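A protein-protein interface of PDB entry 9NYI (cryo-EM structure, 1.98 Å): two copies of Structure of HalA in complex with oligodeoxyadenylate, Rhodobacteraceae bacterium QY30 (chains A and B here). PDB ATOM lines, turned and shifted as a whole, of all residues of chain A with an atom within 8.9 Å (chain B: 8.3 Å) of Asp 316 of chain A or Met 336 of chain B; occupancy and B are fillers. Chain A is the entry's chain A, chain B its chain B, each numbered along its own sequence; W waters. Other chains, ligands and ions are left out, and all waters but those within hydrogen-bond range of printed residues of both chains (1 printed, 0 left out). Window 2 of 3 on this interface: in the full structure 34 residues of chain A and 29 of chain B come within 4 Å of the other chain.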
ATOM      1  N   VAL A 302       4.406   6.055 -38.848  1.00  0.00           N
ATOM      2  CA  VAL A 302       3.160   6.819 -38.865  1.00  0.00           C
ATOM      3  C   VAL A 302       3.090   7.759 -37.665  1.00  0.00           C
ATOM      4  O   VAL A 302       2.622   8.900 -37.774  1.00  0.00           O
ATOM      5  CB  VAL A 302       1.948   5.869 -38.922  1.00  0.00           C
ATOM      6  CG1 VAL A 302       0.659   6.662 -38.978  1.00  0.00           C
ATOM      7  CG2 VAL A 302       2.049   4.963 -40.136  1.00  0.00           C
ATOM      8  N   ALA A 303       3.563   7.300 -36.502  1.00  0.00           N
ATOM      9  CA  ALA A 303       3.550   8.138 -35.308  1.00  0.00           C
ATOM     10  C   ALA A 303       4.499   9.322 -35.448  1.00  0.00           C
ATOM     11  O   ALA A 303       4.181  10.437 -35.017  1.00  0.00           O
ATOM     12  CB  ALA A 303       3.912   7.305 -34.080  1.00  0.00           C
ATOM     13  N   TYR A 304       5.672   9.097 -36.042  1.00  0.00           N
ATOM     14  CA  TYR A 304       6.591  10.198 -36.309  1.00  0.00           C
ATOM     15  C   TYR A 304       5.968  11.202 -37.264  1.00  0.00           C
ATOM     16  O   TYR A 304       6.225  12.407 -37.162  1.00  0.00           O
ATOM     17  CB  TYR A 304       7.906   9.664 -36.876  1.00  0.00           C
ATOM     18  CG  TYR A 304       8.830  10.749 -37.382  1.00  0.00           C
ATOM     19  CD1 TYR A 304       9.482  11.599 -36.500  1.00  0.00           C
ATOM     20  CD2 TYR A 304       9.046  10.925 -38.742  1.00  0.00           C
ATOM     21  CE1 TYR A 304      10.327  12.594 -36.957  1.00  0.00           C
ATOM     22  CE2 TYR A 304       9.889  11.917 -39.210  1.00  0.00           C
ATOM     23  CZ  TYR A 304      10.526  12.748 -38.313  1.00  0.00           C
ATOM     24  OH  TYR A 304      11.365  13.736 -38.774  1.00  0.00           O
ATOM     25  N   TYR A 306       2.713  11.808 -37.580  1.00  0.00           N
ATOM     26  CA  TYR A 306       1.771  12.534 -36.732  1.00  0.00           C
ATOM     27  C   TYR A 306       2.479  13.623 -35.937  1.00  0.00           C
ATOM     28  O   TYR A 306       2.037  14.778 -35.915  1.00  0.00           O
ATOM     29  CB  TYR A 306       1.066  11.572 -35.771  1.00  0.00           C
ATOM     30  CG  TYR A 306       0.011  10.686 -36.392  1.00  0.00           C
ATOM     31  CD1 TYR A 306      -0.894  11.185 -37.320  1.00  0.00           C
ATOM     32  CD2 TYR A 306      -0.089   9.348 -36.037  1.00  0.00           C
ATOM     33  CE1 TYR A 306      -1.860  10.371 -37.883  1.00  0.00           C
ATOM     34  CE2 TYR A 306      -1.049   8.528 -36.591  1.00  0.00           C
ATOM     35  CZ  TYR A 306      -1.932   9.044 -37.515  1.00  0.00           C
ATOM     36  OH  TYR A 306      -2.891   8.229 -38.070  1.00  0.00           O
ATOM     37  N   HIS A 307       3.594  13.271 -35.294  1.00  0.00           N
ATOM     38  CA  HIS A 307       4.274  14.203 -34.401  1.00  0.00           C
ATOM     39  C   HIS A 307       4.897  15.360 -35.172  1.00  0.00           C
ATOM     40  O   HIS A 307       4.862  16.509 -34.717  1.00  0.00           O
ATOM     41  CB  HIS A 307       5.339  13.466 -33.588  1.00  0.00           C
ATOM     42  CG  HIS A 307       6.312  14.375 -32.903  1.00  0.00           C
ATOM     43  ND1 HIS A 307       5.998  15.068 -31.755  1.00  0.00           N
ATOM     44  CD2 HIS A 307       7.584  14.717 -33.213  1.00  0.00           C
ATOM     45  CE1 HIS A 307       7.039  15.789 -31.378  1.00  0.00           C
ATOM     46  NE2 HIS A 307       8.014  15.597 -32.249  1.00  0.00           N
ATOM     47  N   PHE A 310       1.340  17.197 -37.423  1.00  0.00           N
ATOM     48  CA  PHE A 310       0.148  17.680 -36.741  1.00  0.00           C
ATOM     49  C   PHE A 310       0.408  18.007 -35.274  1.00  0.00           C
ATOM     50  O   PHE A 310      -0.543  18.154 -34.498  1.00  0.00           O
ATOM     51  CB  PHE A 310      -0.985  16.667 -36.887  1.00  0.00           C
ATOM     52  CG  PHE A 310      -1.271  16.287 -38.313  1.00  0.00           C
ATOM     53  CD1 PHE A 310      -2.095  17.073 -39.104  1.00  0.00           C
ATOM     54  CD2 PHE A 310      -0.691  15.161 -38.872  1.00  0.00           C
ATOM     55  CE1 PHE A 310      -2.367  16.720 -40.411  1.00  0.00           C
ATOM     56  CE2 PHE A 310      -0.947  14.812 -40.185  1.00  0.00           C
ATOM     57  CZ  PHE A 310      -1.779  15.596 -40.957  1.00  0.00           C
ATOM     58  N   ASN A 311       1.679  18.129 -34.884  1.00  0.00           N
ATOM     59  CA  ASN A 311       2.066  18.626 -33.562  1.00  0.00           C
ATOM     60  C   ASN A 311       1.453  17.788 -32.441  1.00  0.00           C
ATOM     61  O   ASN A 311       0.848  18.309 -31.500  1.00  0.00           O
ATOM     62  CB  ASN A 311       1.702  20.104 -33.409  1.00  0.00           C
ATOM     63  CG  ASN A 311       2.247  20.956 -34.536  1.00  0.00           C
ATOM     64  OD1 ASN A 311       1.500  21.412 -35.402  1.00  0.00           O
ATOM     65  ND2 ASN A 311       3.557  21.172 -34.534  1.00  0.00           N
ATOM     66  N   LEU A 312       1.608  16.475 -32.552  1.00  0.00           N
ATOM     67  CA  LEU A 312       1.166  15.625 -31.459  1.00  0.00           C
ATOM     68  C   LEU A 312       2.367  15.126 -30.668  1.00  0.00           C
ATOM     69  O   LEU A 312       3.377  14.732 -31.260  1.00  0.00           O
ATOM     70  CB  LEU A 312       0.370  14.429 -31.984  1.00  0.00           C
ATOM     71  CG  LEU A 312      -1.143  14.621 -32.113  1.00  0.00           C
ATOM     72  CD1 LEU A 312      -1.821  13.313 -32.486  1.00  0.00           C
ATOM     73  CD2 LEU A 312      -1.728  15.183 -30.826  1.00  0.00           C
ATOM     74  N   PRO A 313       2.297  15.150 -29.338  1.00  0.00           N
ATOM     75  CA  PRO A 313       3.423  14.671 -28.544  1.00  0.00           C
ATOM     76  C   PRO A 313       3.700  13.211 -28.835  1.00  0.00           C
ATOM     77  O   PRO A 313       2.780  12.440 -29.171  1.00  0.00           O
ATOM     78  CB  PRO A 313       2.954  14.884 -27.097  1.00  0.00           C
ATOM     79  CG  PRO A 313       1.476  15.080 -27.177  1.00  0.00           C
ATOM     80  CD  PRO A 313       1.223  15.710 -28.503  1.00  0.00           C
ATOM     81  N   PRO A 314       4.962  12.783 -28.734  1.00  0.00           N
ATOM     82  CA  PRO A 314       5.302  11.408 -29.144  1.00  0.00           C
ATOM     83  C   PRO A 314       4.596  10.341 -28.327  1.00  0.00           C
ATOM     84  O   PRO A 314       4.181   9.310 -28.876  1.00  0.00           O
ATOM     85  CB  PRO A 314       6.826  11.357 -28.963  1.00  0.00           C
ATOM     86  CG  PRO A 314       7.136  12.450 -27.991  1.00  0.00           C
ATOM     87  CD  PRO A 314       6.141  13.533 -28.270  1.00  0.00           C
ATOM     88  N   GLU A 315       4.419  10.584 -27.026  1.00  0.00           N
ATOM     89  CA  GLU A 315       3.887   9.596 -26.096  1.00  0.00           C
ATOM     90  C   GLU A 315       2.420   9.274 -26.338  1.00  0.00           C
ATOM     91  O   GLU A 315       1.892   8.385 -25.660  1.00  0.00           O
ATOM     92  CB  GLU A 315       4.080  10.075 -24.653  1.00  0.00           C
ATOM     93  CG  GLU A 315       3.585  11.494 -24.416  1.00  0.00           C
ATOM     94  CD  GLU A 315       4.669  12.520 -24.664  1.00  0.00           C
ATOM     95  OE1 GLU A 315       5.756  12.113 -25.118  1.00  0.00           O
ATOM     96  OE2 GLU A 315       4.434  13.724 -24.423  1.00  0.00           O
ATOM     97  N   ASP A 316       1.747   9.990 -27.242  1.00  0.00           N
ATOM     98  CA  ASP A 316       0.421   9.595 -27.684  1.00  0.00           C
ATOM     99  C   ASP A 316       0.245   9.649 -29.194  1.00  0.00           C
ATOM    100  O   ASP A 316      -0.760   9.135 -29.694  1.00  0.00           O
ATOM    101  CB  ASP A 316      -0.668  10.430 -26.984  1.00  0.00           C
ATOM    102  CG  ASP A 316      -0.512  11.920 -27.204  1.00  0.00           C
ATOM    103  OD1 ASP A 316       0.153  12.329 -28.176  1.00  0.00           O
ATOM    104  OD2 ASP A 316      -1.048  12.691 -26.378  1.00  0.00           O
ATOM    105  N   ALA A 317       1.191  10.228 -29.938  1.00  0.00           N
ATOM    106  CA  ALA A 317       1.273   9.927 -31.362  1.00  0.00           C
ATOM    107  C   ALA A 317       1.539   8.443 -31.569  1.00  0.00           C
ATOM    108  O   ALA A 317       0.936   7.807 -32.443  1.00  0.00           O
ATOM    109  CB  ALA A 317       2.363  10.771 -32.021  1.00  0.00           C
ATOM    110  N   MET A 318       2.367   7.872 -30.696  1.00  0.00           N
ATOM    111  CA  MET A 318       2.578   6.406 -30.770  1.00  0.00           C
ATOM    112  C   MET A 318       1.246   5.707 -30.476  1.00  0.00           C
ATOM    113  O   MET A 318       0.963   4.701 -31.154  1.00  0.00           O
ATOM    114  CB  MET A 318       3.629   5.955 -29.750  1.00  0.00           C
ATOM    115  CG  MET A 318       4.221   4.591 -30.044  1.00  0.00           C
ATOM    116  SD  MET A 318       4.650   4.380 -31.783  1.00  0.00           S
ATOM    117  CE  MET A 318       6.233   5.232 -31.826  1.00  0.00           C
ATOM    118  N   VAL A 319       0.438   6.246 -29.552  1.00  0.00           N
ATOM    119  CA  VAL A 319      -0.782   5.555 -29.148  1.00  0.00           C
ATOM    120  C   VAL A 319      -1.834   5.644 -30.245  1.00  0.00           C
ATOM    121  O   VAL A 319      -2.516   4.662 -30.553  1.00  0.00           O
ATOM    122  CB  VAL A 319      -1.291   6.117 -27.807  1.00  0.00           C
ATOM    123  CG1 VAL A 319      -2.750   5.760 -27.586  1.00  0.00           C
ATOM    124  CG2 VAL A 319      -0.437   5.596 -26.662  1.00  0.00           C
ATOM    125  N   LYS A 320      -1.973   6.819 -30.862  1.00  0.00           N
ATOM    126  CA  LYS A 320      -2.863   6.958 -32.009  1.00  0.00           C
ATOM    127  C   LYS A 320      -2.430   6.051 -33.156  1.00  0.00           C
ATOM    128  O   LYS A 320      -3.274   5.428 -33.817  1.00  0.00           O
ATOM    129  CB  LYS A 320      -2.902   8.417 -32.463  1.00  0.00           C
ATOM    130  CG  LYS A 320      -3.434   8.614 -33.869  1.00  0.00           C
ATOM    131  CD  LYS A 320      -3.361  10.068 -34.284  1.00  0.00           C
ATOM    132  CE  LYS A 320      -4.744  10.660 -34.445  1.00  0.00           C
ATOM    133  NZ  LYS A 320      -4.797  11.614 -35.584  1.00  0.00           N
ATOM    134  N   ALA A 321      -1.121   5.962 -33.404  1.00  0.00           N
ATOM    135  CA  ALA A 321      -0.635   5.116 -34.488  1.00  0.00           C
ATOM    136  C   ALA A 321      -0.975   3.650 -34.245  1.00  0.00           C
ATOM    137  O   ALA A 321      -1.470   2.966 -35.148  1.00  0.00           O
ATOM    138  CB  ALA A 321       0.870   5.300 -34.667  1.00  0.00           C
ATOM    139  N   THR A 322      -0.729   3.150 -33.030  1.00  0.00           N
ATOM    140  CA  THR A 322      -1.060   1.753 -32.745  1.00  0.00           C
ATOM    141  C   THR A 322      -2.563   1.533 -32.628  1.00  0.00           C
ATOM    142  O   THR A 322      -3.027   0.389 -32.625  1.00  0.00           O
ATOM    143  CB  THR A 322      -0.376   1.289 -31.457  1.00  0.00           C
ATOM    144  OG1 THR A 322      -0.846  -0.020 -31.112  1.00  0.00           O
ATOM    145  CG2 THR A 322      -0.675   2.236 -30.330  1.00  0.00           C
ATOM    146  N   GLU A 323      -3.320   2.600 -32.368  1.00  0.00           N
ATOM    147  CA  GLU A 323      -4.772   2.503 -32.249  1.00  0.00           C
ATOM    148  C   GLU A 323      -5.434   2.402 -33.613  1.00  0.00           C
ATOM    149  O   GLU A 323      -6.466   1.739 -33.768  1.00  0.00           O
ATOM    150  CB  GLU A 323      -5.321   3.702 -31.474  1.00  0.00           C
ATOM    151  CG  GLU A 323      -5.765   3.346 -30.072  1.00  0.00           C
ATOM    152  CD  GLU A 323      -6.206   4.568 -29.288  1.00  0.00           C
ATOM    153  OE1 GLU A 323      -5.469   5.575 -29.288  1.00  0.00           O
ATOM    154  OE2 GLU A 323      -7.291   4.523 -28.672  1.00  0.00           O
ATOM    155  N   ILE A 324      -4.867   3.079 -34.608  1.00  0.00           N
ATOM    156  CA  ILE A 324      -5.404   2.997 -35.961  1.00  0.00           C
ATOM    157  C   ILE A 324      -4.815   1.805 -36.705  1.00  0.00           C
ATOM    158  O   ILE A 324      -5.469   1.212 -37.570  1.00  0.00           O
ATOM    159  CB  ILE A 324      -5.160   4.335 -36.682  1.00  0.00           C
ATOM    160  CG1 ILE A 324      -6.058   5.396 -36.051  1.00  0.00           C
ATOM    161  CG2 ILE A 324      -5.380   4.227 -38.191  1.00  0.00           C
ATOM    162  CD1 ILE A 324      -5.766   6.799 -36.489  1.00  0.00           C
ATOM    163  N   ASN A 332     -12.496   6.675 -33.871  1.00  0.00           N
ATOM    164  CA  ASN A 332     -12.262   7.787 -32.961  1.00  0.00           C
ATOM    165  C   ASN A 332     -11.417   8.892 -33.587  1.00  0.00           C
ATOM    166  O   ASN A 332     -11.494  10.040 -33.137  1.00  0.00           O
ATOM    167  CB  ASN A 332     -11.596   7.290 -31.676  1.00  0.00           C
ATOM    168  CG  ASN A 332     -12.603   6.916 -30.606  1.00  0.00           C
ATOM    169  OD1 ASN A 332     -13.793   7.200 -30.733  1.00  0.00           O
ATOM    170  ND2 ASN A 332     -12.129   6.273 -29.546  1.00  0.00           N
ATOM    171  N   TYR A 333     -10.624   8.582 -34.612  1.00  0.00           N
ATOM    172  CA  TYR A 333      -9.719   9.561 -35.194  1.00  0.00           C
ATOM    173  C   TYR A 333      -9.989   9.876 -36.658  1.00  0.00           C
ATOM    174  O   TYR A 333      -9.441  10.860 -37.167  1.00  0.00           O
ATOM    175  CB  TYR A 333      -8.264   9.092 -35.058  1.00  0.00           C
ATOM    176  CG  TYR A 333      -7.838   8.790 -33.641  1.00  0.00           C
ATOM    177  CD1 TYR A 333      -7.583   9.812 -32.737  1.00  0.00           C
ATOM    178  CD2 TYR A 333      -7.685   7.480 -33.208  1.00  0.00           C
ATOM    179  CE1 TYR A 333      -7.190   9.539 -31.444  1.00  0.00           C
ATOM    180  CE2 TYR A 333      -7.293   7.197 -31.916  1.00  0.00           C
ATOM    181  CZ  TYR A 333      -7.046   8.230 -31.038  1.00  0.00           C
ATOM    182  OH  TYR A 333      -6.656   7.950 -29.749  1.00  0.00           O
ATOM    183  N   ASP A 340      -5.596  15.299 -41.366  1.00  0.00           N
ATOM    184  CA  ASP A 340      -4.916  14.026 -41.170  1.00  0.00           C
ATOM    185  C   ASP A 340      -5.733  12.827 -41.640  1.00  0.00           C
ATOM    186  O   ASP A 340      -5.342  11.686 -41.374  1.00  0.00           O
ATOM    187  CB  ASP A 340      -4.521  13.866 -39.695  1.00  0.00           C
ATOM    188  CG  ASP A 340      -5.705  13.552 -38.784  1.00  0.00           C
ATOM    189  OD1 ASP A 340      -6.870  13.648 -39.225  1.00  0.00           O
ATOM    190  OD2 ASP A 340      -5.462  13.203 -37.611  1.00  0.00           O
ATOM    191  N   TYR B 330     -14.618  -0.726 -28.213  1.00  0.00           N
ATOM    192  CA  TYR B 330     -13.459   0.055 -27.790  1.00  0.00           C
ATOM    193  C   TYR B 330     -13.716   1.554 -27.908  1.00  0.00           C
ATOM    194  O   TYR B 330     -13.449   2.315 -26.970  1.00  0.00           O
ATOM    195  CB  TYR B 330     -12.227  -0.346 -28.600  1.00  0.00           C
ATOM    196  CG  TYR B 330     -11.003   0.477 -28.275  1.00  0.00           C
ATOM    197  CD1 TYR B 330     -10.212   0.169 -27.178  1.00  0.00           C
ATOM    198  CD2 TYR B 330     -10.634   1.558 -29.064  1.00  0.00           C
ATOM    199  CE1 TYR B 330      -9.093   0.915 -26.872  1.00  0.00           C
ATOM    200  CE2 TYR B 330      -9.513   2.307 -28.767  1.00  0.00           C
ATOM    201  CZ  TYR B 330      -8.745   1.978 -27.671  1.00  0.00           C
ATOM    202  OH  TYR B 330      -7.630   2.719 -27.363  1.00  0.00           O
ATOM    203  N   TYR B 333     -15.535   3.866 -25.266  1.00  0.00           N
ATOM    204  CA  TYR B 333     -14.920   4.203 -23.993  1.00  0.00           C
ATOM    205  C   TYR B 333     -13.547   4.849 -24.106  1.00  0.00           C
ATOM    206  O   TYR B 333     -13.057   5.388 -23.108  1.00  0.00           O
ATOM    207  CB  TYR B 333     -14.797   2.953 -23.110  1.00  0.00           C
ATOM    208  CG  TYR B 333     -16.102   2.233 -22.867  1.00  0.00           C
ATOM    209  CD1 TYR B 333     -17.049   2.746 -21.992  1.00  0.00           C
ATOM    210  CD2 TYR B 333     -16.384   1.036 -23.509  1.00  0.00           C
ATOM    211  CE1 TYR B 333     -18.241   2.088 -21.764  1.00  0.00           C
ATOM    212  CE2 TYR B 333     -17.573   0.371 -23.289  1.00  0.00           C
ATOM    213  CZ  TYR B 333     -18.497   0.901 -22.416  1.00  0.00           C
ATOM    214  OH  TYR B 333     -19.684   0.240 -22.195  1.00  0.00           O
ATOM    215  N   ALA B 334     -12.915   4.815 -25.275  1.00  0.00           N
ATOM    216  CA  ALA B 334     -11.559   5.324 -25.436  1.00  0.00           C
ATOM    217  C   ALA B 334     -11.606   6.778 -25.885  1.00  0.00           C
ATOM    218  O   ALA B 334     -12.189   7.095 -26.927  1.00  0.00           O
ATOM    219  CB  ALA B 334     -10.782   4.477 -26.441  1.00  0.00           C
ATOM    220  N   LYS B 335     -10.989   7.658 -25.099  1.00  0.00           N
ATOM    221  CA  LYS B 335     -10.905   9.078 -25.419  1.00  0.00           C
ATOM    222  C   LYS B 335      -9.540   9.582 -24.984  1.00  0.00           C
ATOM    223  O   LYS B 335      -9.173   9.440 -23.814  1.00  0.00           O
ATOM    224  CB  LYS B 335     -12.019   9.868 -24.729  1.00  0.00           C
ATOM    225  CG  LYS B 335     -12.306  11.208 -25.369  1.00  0.00           C
ATOM    226  CD  LYS B 335     -13.518  11.872 -24.737  1.00  0.00           C
ATOM    227  CE  LYS B 335     -13.537  13.366 -25.012  1.00  0.00           C
ATOM    228  NZ  LYS B 335     -14.803  13.992 -24.540  1.00  0.00           N
ATOM    229  N   MET B 336      -8.792  10.167 -25.917  1.00  0.00           N
ATOM    230  CA  MET B 336      -7.440  10.608 -25.603  1.00  0.00           C
ATOM    231  C   MET B 336      -7.491  11.773 -24.622  1.00  0.00           C
ATOM    232  O   MET B 336      -8.271  12.715 -24.795  1.00  0.00           O
ATOM    233  CB  MET B 336      -6.697  11.016 -26.875  1.00  0.00           C
ATOM    234  CG  MET B 336      -5.336  11.634 -26.597  1.00  0.00           C
ATOM    235  SD  MET B 336      -4.174  11.413 -27.958  1.00  0.00           S
ATOM    236  CE  MET B 336      -5.043  12.259 -29.277  1.00  0.00           C
ATOM    237  N   GLY B 337      -6.660  11.704 -23.585  1.00  0.00           N
ATOM    238  CA  GLY B 337      -6.618  12.718 -22.555  1.00  0.00           C
ATOM    239  C   GLY B 337      -7.470  12.426 -21.339  1.00  0.00           C
ATOM    240  O   GLY B 337      -7.432  13.204 -20.378  1.00  0.00           O
ATOM    241  N   GLN B 338      -8.234  11.340 -21.351  1.00  0.00           N
ATOM    242  CA  GLN B 338      -9.033  10.943 -20.202  1.00  0.00           C
ATOM    243  C   GLN B 338      -8.184  10.168 -19.197  1.00  0.00           C
ATOM    244  O   GLN B 338      -7.125   9.628 -19.523  1.00  0.00           O
ATOM    245  CB  GLN B 338     -10.233  10.105 -20.646  1.00  0.00           C
ATOM    246  CG  GLN B 338     -11.540  10.881 -20.710  1.00  0.00           C
ATOM    247  CD  GLN B 338     -12.760   9.982 -20.650  1.00  0.00           C
ATOM    248  OE1 GLN B 338     -12.641   8.763 -20.531  1.00  0.00           O
ATOM    249  NE2 GLN B 338     -13.941  10.581 -20.734  1.00  0.00           N
ATOM    250  N   GLU B 339      -8.669  10.123 -17.953  1.00  0.00           N
ATOM    251  CA  GLU B 339      -7.911   9.481 -16.882  1.00  0.00           C
ATOM    252  C   GLU B 339      -7.730   7.990 -17.138  1.00  0.00           C
ATOM    253  O   GLU B 339      -6.652   7.436 -16.890  1.00  0.00           O
ATOM    254  CB  GLU B 339      -8.603   9.714 -15.539  1.00  0.00           C
ATOM    255  CG  GLU B 339      -8.804  11.178 -15.188  1.00  0.00           C
ATOM    256  CD  GLU B 339      -7.494  11.910 -14.967  1.00  0.00           C
ATOM    257  OE1 GLU B 339      -6.537  11.280 -14.467  1.00  0.00           O
ATOM    258  OE2 GLU B 339      -7.421  13.113 -15.291  1.00  0.00           O
ATOM    259  N   ASP B 340      -8.770   7.322 -17.631  1.00  0.00           N
ATOM    260  CA  ASP B 340      -8.745   5.882 -17.847  1.00  0.00           C
ATOM    261  C   ASP B 340      -8.291   5.490 -19.249  1.00  0.00           C
ATOM    262  O   ASP B 340      -8.390   4.313 -19.610  1.00  0.00           O
ATOM    263  CB  ASP B 340     -10.125   5.283 -17.538  1.00  0.00           C
ATOM    264  CG  ASP B 340     -11.166   5.584 -18.613  1.00  0.00           C
ATOM    265  OD1 ASP B 340     -10.912   6.417 -19.509  1.00  0.00           O
ATOM    266  OD2 ASP B 340     -12.254   4.974 -18.559  1.00  0.00           O
ATOM    267  N   PHE B 341      -7.798   6.445 -20.040  1.00  0.00           N
ATOM    268  CA  PHE B 341      -7.464   6.161 -21.433  1.00  0.00           C
ATOM    269  C   PHE B 341      -6.337   5.139 -21.546  1.00  0.00           C
ATOM    270  O   PHE B 341      -6.407   4.218 -22.368  1.00  0.00           O
ATOM    271  CB  PHE B 341      -7.099   7.459 -22.152  1.00  0.00           C
ATOM    272  CG  PHE B 341      -6.707   7.265 -23.585  1.00  0.00           C
ATOM    273  CD1 PHE B 341      -7.597   6.718 -24.496  1.00  0.00           C
ATOM    274  CD2 PHE B 341      -5.445   7.622 -24.021  1.00  0.00           C
ATOM    275  CE1 PHE B 341      -7.231   6.535 -25.817  1.00  0.00           C
ATOM    276  CE2 PHE B 341      -5.076   7.444 -25.336  1.00  0.00           C
ATOM    277  CZ  PHE B 341      -5.967   6.895 -26.237  1.00  0.00           C
ATOM    278  N   HIS B 342      -5.289   5.281 -20.729  1.00  0.00           N
ATOM    279  CA  HIS B 342      -4.197   4.313 -20.756  1.00  0.00           C
ATOM    280  C   HIS B 342      -4.675   2.927 -20.340  1.00  0.00           C
ATOM    281  O   HIS B 342      -4.266   1.919 -20.928  1.00  0.00           O
ATOM    282  CB  HIS B 342      -3.054   4.783 -19.857  1.00  0.00           C
ATOM    283  CG  HIS B 342      -2.355   6.008 -20.357  1.00  0.00           C
ATOM    284  ND1 HIS B 342      -2.347   6.368 -21.687  1.00  0.00           N
ATOM    285  CD2 HIS B 342      -1.646   6.960 -19.705  1.00  0.00           C
ATOM    286  CE1 HIS B 342      -1.662   7.488 -21.834  1.00  0.00           C
ATOM    287  NE2 HIS B 342      -1.225   7.867 -20.646  1.00  0.00           N
HETATM  288  O   HOH W   1      -3.424   8.898 -28.719  1.00  0.00           O
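The side-chain amide nitrogen of Asn 332 of chain A sits at hydrogen-bond distance from the backbone carbonyl oxygen of Ala 334 of chain B, at 2.7 Å. OE2 of Glu 323 of chain A lies close to OH of Tyr 330 of chain B (2.3 Å). The side-chain sulfur (SD) of Met 336 of chain B lies close to the side-chain carboxylate (OD2) of Asp 316 of chain A (3.7 Å).
OE1 of Glu 323 of chain A is in hydrogen-bond range of OH of Tyr 333 of chain A (2.7 Å).
Among the printed residues, merely in contact across the chains: Glu 323 of chain A with Phe 341 of chain B (3.4 Å), Val 319 of chain A with Phe 341 of chain B (3.6 Å) and Tyr 333 of chain A with Phe 341 of chain B (3.7 Å).
No residue of chain B comes within 4 Å of Pro 313 of chain A. No residue of chain B comes within 4 Å of Ala 317 of chain A. Printed residues of chain B within 4 Å of Val 319 of chain A: Phe 341 (3.6 Å). Printed residues of chain B within 4 Å of Tyr 333 of chain A: Phe 341 (3.7 Å). Printed residues of chain A within 4 Å of Ala 334 of chain B: Asn 332. Of chain A, only Asp 316 comes within 4 Å of Met 336 of chain B. No residue of chain A comes within 4 Å of Gly 337 of chain B. Printed residues of chain A within 4 Å of Phe 341 of chain B: Val 319 (3.6 Å), Glu 323 (3.4 Å) and Tyr 333 (3.7 Å). The nearest printed residue of chain B that does not touch Glu 323 of chain A is Ala 334 of chain B (4.1 Å).
Of the 23 printed residues of chain A, 5 touch a printed residue of chain B. Printed residues of chain A that touch a printed residue of chain B: Asp 316, Val 319, Glu 323, Asn 332 and Tyr 333. Hydrophobic or aromatic side chains of chain B within 4 Å of the printed part of chain A: Tyr 330, Ala 334, Met 336 and Phe 341. Among the printed residues, 6 pairs touch across the chains.
2 positions are printed for both chains. Of the 6 pairs that touch across the chains among the printed residues, none has its exchanged pair printed and touching as well.
Water W1 lies within hydrogen-bond range of SD of Met 336 of chain B, O of Asp 316 of chain A and N of Lys 320 of chain A.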
